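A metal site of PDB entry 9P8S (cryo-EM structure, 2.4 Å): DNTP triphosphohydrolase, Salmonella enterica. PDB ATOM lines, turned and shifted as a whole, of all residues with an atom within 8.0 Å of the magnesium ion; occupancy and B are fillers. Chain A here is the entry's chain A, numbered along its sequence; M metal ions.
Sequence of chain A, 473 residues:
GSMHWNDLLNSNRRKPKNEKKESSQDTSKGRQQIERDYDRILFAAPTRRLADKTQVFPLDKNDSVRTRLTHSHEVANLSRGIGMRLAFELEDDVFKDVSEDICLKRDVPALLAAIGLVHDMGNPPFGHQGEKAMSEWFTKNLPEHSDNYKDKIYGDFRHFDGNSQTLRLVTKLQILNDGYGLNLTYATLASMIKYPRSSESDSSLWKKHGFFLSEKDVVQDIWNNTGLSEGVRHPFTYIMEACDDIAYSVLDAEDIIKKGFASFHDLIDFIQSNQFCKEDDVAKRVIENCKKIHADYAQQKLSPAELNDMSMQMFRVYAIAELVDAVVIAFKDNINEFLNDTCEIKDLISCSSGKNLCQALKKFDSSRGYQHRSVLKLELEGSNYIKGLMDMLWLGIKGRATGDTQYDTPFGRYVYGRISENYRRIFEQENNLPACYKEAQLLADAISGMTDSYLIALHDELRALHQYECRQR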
ATOM      1  N   GLN A  55     -20.357  21.838  -8.258  1.00  0.00           N
ATOM      2  CA  GLN A  55     -20.910  23.137  -8.634  1.00  0.00           C
ATOM      3  C   GLN A  55     -20.062  24.278  -8.075  1.00  0.00           C
ATOM      4  O   GLN A  55     -19.488  25.070  -8.838  1.00  0.00           O
ATOM      5  CB  GLN A  55     -22.363  23.243  -8.157  1.00  0.00           C
ATOM      6  CG  GLN A  55     -22.904  24.653  -8.068  1.00  0.00           C
ATOM      7  CD  GLN A  55     -23.298  25.203  -9.424  1.00  0.00           C
ATOM      8  OE1 GLN A  55     -23.263  24.493 -10.432  1.00  0.00           O
ATOM      9  NE2 GLN A  55     -23.680  26.472  -9.462  1.00  0.00           N
ATOM     10  N   ARG A  68     -24.074  20.148  -9.677  1.00  0.00           N
ATOM     11  CA  ARG A  68     -24.527  20.677 -10.959  1.00  0.00           C
ATOM     12  C   ARG A  68     -25.964  20.259 -11.244  1.00  0.00           C
ATOM     13  O   ARG A  68     -26.734  21.028 -11.822  1.00  0.00           O
ATOM     14  CB  ARG A  68     -23.604  20.223 -12.082  1.00  0.00           C
ATOM     15  CG  ARG A  68     -22.342  21.049 -12.206  1.00  0.00           C
ATOM     16  CD  ARG A  68     -21.884  21.140 -13.654  1.00  0.00           C
ATOM     17  NE  ARG A  68     -20.480  21.514 -13.761  1.00  0.00           N
ATOM     18  CZ  ARG A  68     -20.001  22.736 -13.513  1.00  0.00           C
ATOM     19  NH1 ARG A  68     -20.796  23.723 -13.142  1.00  0.00           N
ATOM     20  NH2 ARG A  68     -18.697  22.957 -13.638  1.00  0.00           N
ATOM     21  N   HIS A  71     -28.360  22.301  -8.903  1.00  0.00           N
ATOM     22  CA  HIS A  71     -28.375  23.682  -9.383  1.00  0.00           C
ATOM     23  C   HIS A  71     -29.147  23.801 -10.690  1.00  0.00           C
ATOM     24  O   HIS A  71     -29.926  24.750 -10.873  1.00  0.00           O
ATOM     25  CB  HIS A  71     -26.937  24.174  -9.566  1.00  0.00           C
ATOM     26  CG  HIS A  71     -26.815  25.346 -10.496  1.00  0.00           C
ATOM     27  ND1 HIS A  71     -27.060  26.639 -10.097  1.00  0.00           N
ATOM     28  CD2 HIS A  71     -26.461  25.412 -11.801  1.00  0.00           C
ATOM     29  CE1 HIS A  71     -26.869  27.454 -11.122  1.00  0.00           C
ATOM     30  NE2 HIS A  71     -26.505  26.730 -12.169  1.00  0.00           N
ATOM     31  N   SER A  72     -28.961  22.856 -11.609  1.00  0.00           N
ATOM     32  CA  SER A  72     -29.686  22.878 -12.864  1.00  0.00           C
ATOM     33  C   SER A  72     -31.188  22.725 -12.631  1.00  0.00           C
ATOM     34  O   SER A  72     -31.986  23.409 -13.278  1.00  0.00           O
ATOM     35  CB  SER A  72     -29.181  21.771 -13.785  1.00  0.00           C
ATOM     36  OG  SER A  72     -27.800  21.927 -14.044  1.00  0.00           O
ATOM     37  N   VAL A  75     -32.517  26.054 -11.281  1.00  0.00           N
ATOM     38  CA  VAL A  75     -32.623  27.027 -12.354  1.00  0.00           C
ATOM     39  C   VAL A  75     -33.822  26.704 -13.245  1.00  0.00           C
ATOM     40  O   VAL A  75     -34.566  27.601 -13.669  1.00  0.00           O
ATOM     41  CB  VAL A  75     -31.318  27.077 -13.166  1.00  0.00           C
ATOM     42  CG1 VAL A  75     -31.489  27.956 -14.397  1.00  0.00           C
ATOM     43  CG2 VAL A  75     -30.189  27.596 -12.308  1.00  0.00           C
ATOM     44  N   GLY A 116     -33.335  25.935 -18.820  1.00  0.00           N
ATOM     45  CA  GLY A 116     -32.729  26.030 -17.504  1.00  0.00           C
ATOM     46  C   GLY A 116     -32.051  24.742 -17.086  1.00  0.00           C
ATOM     47  O   GLY A 116     -30.963  24.758 -16.504  1.00  0.00           O
ATOM     48  N   HIS A 119     -28.732  24.106 -19.258  1.00  0.00           N
ATOM     49  CA  HIS A 119     -27.806  25.218 -19.464  1.00  0.00           C
ATOM     50  C   HIS A 119     -26.385  24.889 -19.051  1.00  0.00           C
ATOM     51  O   HIS A 119     -25.430  25.424 -19.633  1.00  0.00           O
ATOM     52  CB  HIS A 119     -28.309  26.464 -18.725  1.00  0.00           C
ATOM     53  CG  HIS A 119     -27.958  26.481 -17.273  1.00  0.00           C
ATOM     54  ND1 HIS A 119     -28.607  25.712 -16.331  1.00  0.00           N
ATOM     55  CD2 HIS A 119     -27.029  27.201 -16.596  1.00  0.00           C
ATOM     56  CE1 HIS A 119     -28.089  25.942 -15.137  1.00  0.00           C
ATOM     57  NE2 HIS A 119     -27.123  26.841 -15.270  1.00  0.00           N
ATOM     58  N   ASP A 120     -26.197  24.021 -18.053  1.00  0.00           N
ATOM     59  CA  ASP A 120     -24.867  23.684 -17.552  1.00  0.00           C
ATOM     60  C   ASP A 120     -24.490  22.230 -17.846  1.00  0.00           C
ATOM     61  O   ASP A 120     -23.681  21.642 -17.136  1.00  0.00           O
ATOM     62  CB  ASP A 120     -24.764  23.960 -16.062  1.00  0.00           C
ATOM     63  CG  ASP A 120     -24.349  25.387 -15.753  1.00  0.00           C
ATOM     64  OD1 ASP A 120     -23.444  25.902 -16.448  1.00  0.00           O
ATOM     65  OD2 ASP A 120     -24.910  25.989 -14.817  1.00  0.00           O
ATOM     66  N   MET A 121     -25.064  21.658 -18.896  1.00  0.00           N
ATOM     67  CA  MET A 121     -24.866  20.230 -19.151  1.00  0.00           C
ATOM     68  C   MET A 121     -23.467  19.920 -19.665  1.00  0.00           C
ATOM     69  O   MET A 121     -22.941  18.834 -19.396  1.00  0.00           O
ATOM     70  CB  MET A 121     -25.909  19.735 -20.152  1.00  0.00           C
ATOM     71  CG  MET A 121     -25.966  18.231 -20.285  1.00  0.00           C
ATOM     72  SD  MET A 121     -27.124  17.690 -21.561  1.00  0.00           S
ATOM     73  CE  MET A 121     -26.035  17.597 -22.972  1.00  0.00           C
ATOM     74  N   ASN A 123     -20.583  21.756 -19.016  1.00  0.00           N
ATOM     75  CA  ASN A 123     -19.503  22.376 -18.276  1.00  0.00           C
ATOM     76  C   ASN A 123     -18.520  21.309 -17.787  1.00  0.00           C
ATOM     77  O   ASN A 123     -18.929  20.219 -17.399  1.00  0.00           O
ATOM     78  CB  ASN A 123     -20.044  23.173 -17.098  1.00  0.00           C
ATOM     79  CG  ASN A 123     -20.649  24.497 -17.516  1.00  0.00           C
ATOM     80  OD1 ASN A 123     -21.508  24.551 -18.393  1.00  0.00           O
ATOM     81  ND2 ASN A 123     -20.200  25.575 -16.889  1.00  0.00           N
ATOM     82  N   ASN A 163     -20.761  26.843 -22.404  1.00  0.00           N
ATOM     83  CA  ASN A 163     -21.975  26.977 -23.191  1.00  0.00           C
ATOM     84  C   ASN A 163     -21.803  26.385 -24.585  1.00  0.00           C
ATOM     85  O   ASN A 163     -22.689  25.685 -25.093  1.00  0.00           O
ATOM     86  CB  ASN A 163     -22.391  28.447 -23.275  1.00  0.00           C
ATOM     87  CG  ASN A 163     -22.672  29.039 -21.915  1.00  0.00           C
ATOM     88  OD1 ASN A 163     -21.995  29.976 -21.483  1.00  0.00           O
ATOM     89  ND2 ASN A 163     -23.662  28.503 -21.220  1.00  0.00           N
ATOM     90  N   LYS A 194     -26.217  31.269 -25.585  1.00  0.00           N
ATOM     91  CA  LYS A 194     -26.118  32.354 -24.622  1.00  0.00           C
ATOM     92  C   LYS A 194     -25.404  33.569 -25.187  1.00  0.00           C
ATOM     93  O   LYS A 194     -25.796  34.704 -24.900  1.00  0.00           O
ATOM     94  CB  LYS A 194     -25.394  31.864 -23.366  1.00  0.00           C
ATOM     95  CG  LYS A 194     -25.505  32.782 -22.176  1.00  0.00           C
ATOM     96  CD  LYS A 194     -24.789  32.211 -20.967  1.00  0.00           C
ATOM     97  CE  LYS A 194     -24.883  33.130 -19.777  1.00  0.00           C
ATOM     98  NZ  LYS A 194     -24.138  32.587 -18.599  1.00  0.00           N
ATOM     99  N   MET A 240     -33.282  32.901 -18.811  1.00  0.00           N
ATOM    100  CA  MET A 240     -32.482  31.791 -18.299  1.00  0.00           C
ATOM    101  C   MET A 240     -31.226  32.290 -17.603  1.00  0.00           C
ATOM    102  O   MET A 240     -30.855  31.777 -16.543  1.00  0.00           O
ATOM    103  CB  MET A 240     -32.132  30.837 -19.434  1.00  0.00           C
ATOM    104  CG  MET A 240     -31.390  29.589 -18.986  1.00  0.00           C
ATOM    105  SD  MET A 240     -29.604  29.735 -19.195  1.00  0.00           S
ATOM    106  CE  MET A 240     -29.479  29.780 -20.969  1.00  0.00           C
ATOM    107  N   GLU A 241     -30.560  33.291 -18.178  1.00  0.00           N
ATOM    108  CA  GLU A 241     -29.364  33.850 -17.547  1.00  0.00           C
ATOM    109  C   GLU A 241     -29.703  34.529 -16.228  1.00  0.00           C
ATOM    110  O   GLU A 241     -28.947  34.401 -15.250  1.00  0.00           O
ATOM    111  CB  GLU A 241     -28.699  34.834 -18.509  1.00  0.00           C
ATOM    112  CG  GLU A 241     -27.586  35.654 -17.883  1.00  0.00           C
ATOM    113  CD  GLU A 241     -27.031  36.688 -18.836  1.00  0.00           C
ATOM    114  OE1 GLU A 241     -27.817  37.528 -19.333  1.00  0.00           O
ATOM    115  OE2 GLU A 241     -25.813  36.675 -19.103  1.00  0.00           O
ATOM    116  N   CYS A 243     -32.207  33.737 -14.236  1.00  0.00           N
ATOM    117  CA  CYS A 243     -32.475  32.674 -13.275  1.00  0.00           C
ATOM    118  C   CYS A 243     -31.176  32.020 -12.811  1.00  0.00           C
ATOM    119  O   CYS A 243     -31.037  31.678 -11.630  1.00  0.00           O
ATOM    120  CB  CYS A 243     -33.403  31.629 -13.903  1.00  0.00           C
ATOM    121  SG  CYS A 243     -35.084  32.224 -14.183  1.00  0.00           S
ATOM    122  N   ASP A 244     -30.221  31.840 -13.725  1.00  0.00           N
ATOM    123  CA  ASP A 244     -28.922  31.288 -13.346  1.00  0.00           C
ATOM    124  C   ASP A 244     -28.220  32.190 -12.340  1.00  0.00           C
ATOM    125  O   ASP A 244     -27.670  31.707 -11.333  1.00  0.00           O
ATOM    126  CB  ASP A 244     -28.065  31.109 -14.593  1.00  0.00           C
ATOM    127  CG  ASP A 244     -26.971  30.077 -14.409  1.00  0.00           C
ATOM    128  OD1 ASP A 244     -27.057  29.292 -13.439  1.00  0.00           O
ATOM    129  OD2 ASP A 244     -26.030  30.049 -15.231  1.00  0.00           O
ATOM    130  N   ASP A 245     -28.229  33.500 -12.586  1.00  0.00           N
ATOM    131  CA  ASP A 245     -27.585  34.440 -11.663  1.00  0.00           C
ATOM    132  C   ASP A 245     -28.278  34.432 -10.307  1.00  0.00           C
ATOM    133  O   ASP A 245     -27.617  34.469  -9.268  1.00  0.00           O
ATOM    134  CB  ASP A 245     -27.578  35.840 -12.267  1.00  0.00           C
ATOM    135  CG  ASP A 245     -26.532  36.008 -13.338  1.00  0.00           C
ATOM    136  OD1 ASP A 245     -25.770  35.048 -13.586  1.00  0.00           O
ATOM    137  OD2 ASP A 245     -26.466  37.099 -13.939  1.00  0.00           O
ATOM    138  N   ALA A 247     -29.995  31.980  -8.956  1.00  0.00           N
ATOM    139  CA  ALA A 247     -29.682  30.722  -8.291  1.00  0.00           C
ATOM    140  C   ALA A 247     -28.282  30.757  -7.701  1.00  0.00           C
ATOM    141  O   ALA A 247     -28.093  30.433  -6.523  1.00  0.00           O
ATOM    142  CB  ALA A 247     -29.825  29.561  -9.281  1.00  0.00           C
ATOM    143  N   TYR A 248     -27.291  31.158  -8.500  1.00  0.00           N
ATOM    144  CA  TYR A 248     -25.941  31.331  -7.994  1.00  0.00           C
ATOM    145  C   TYR A 248     -25.944  32.163  -6.719  1.00  0.00           C
ATOM    146  O   TYR A 248     -25.629  31.665  -5.630  1.00  0.00           O
ATOM    147  CB  TYR A 248     -25.061  32.007  -9.053  1.00  0.00           C
ATOM    148  CG  TYR A 248     -24.344  31.047  -9.974  1.00  0.00           C
ATOM    149  CD1 TYR A 248     -23.396  30.164  -9.497  1.00  0.00           C
ATOM    150  CD2 TYR A 248     -24.625  31.041 -11.336  1.00  0.00           C
ATOM    151  CE1 TYR A 248     -22.737  29.291 -10.345  1.00  0.00           C
ATOM    152  CE2 TYR A 248     -23.979  30.172 -12.190  1.00  0.00           C
ATOM    153  CZ  TYR A 248     -23.032  29.299 -11.691  1.00  0.00           C
ATOM    154  OH  TYR A 248     -22.381  28.434 -12.538  1.00  0.00           O
HETATM  155 MG    MG M   1     -25.776  27.646 -13.894  1.00  0.00          MG
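OD1 of Asp 120 lies close to OD1 of Asn 123. The backbone carbonyl oxygen (O) of Gly 116 is in hydrogen-bond range of a ring nitrogen (ND1) of His 119, 2.5 Å away. NE2 of Gln 55 sits at hydrogen-bond distance from ND1 of His 71 (3.4 Å).
CE2 of Tyr 248 touches the magnesium ion, 3.5 Å away. Five residues have an atom within 4 Å of the magnesium ion: His 71, His 119, Asp 120, Asp 244 and Tyr 248.
The magnesium ion is bound by OD2 of Asp 120 (2.1 Å), NE2 of His 71 (2.1 Å), NE2 of His 119 (2.1 Å) and OD1 of Asp 244 (2.1 Å). The magnesium ion has four donor atoms within binding distance. Slightly farther from the magnesium ion lies the side-chain carboxylate (OD2) of Asp 244 (2.8 Å).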
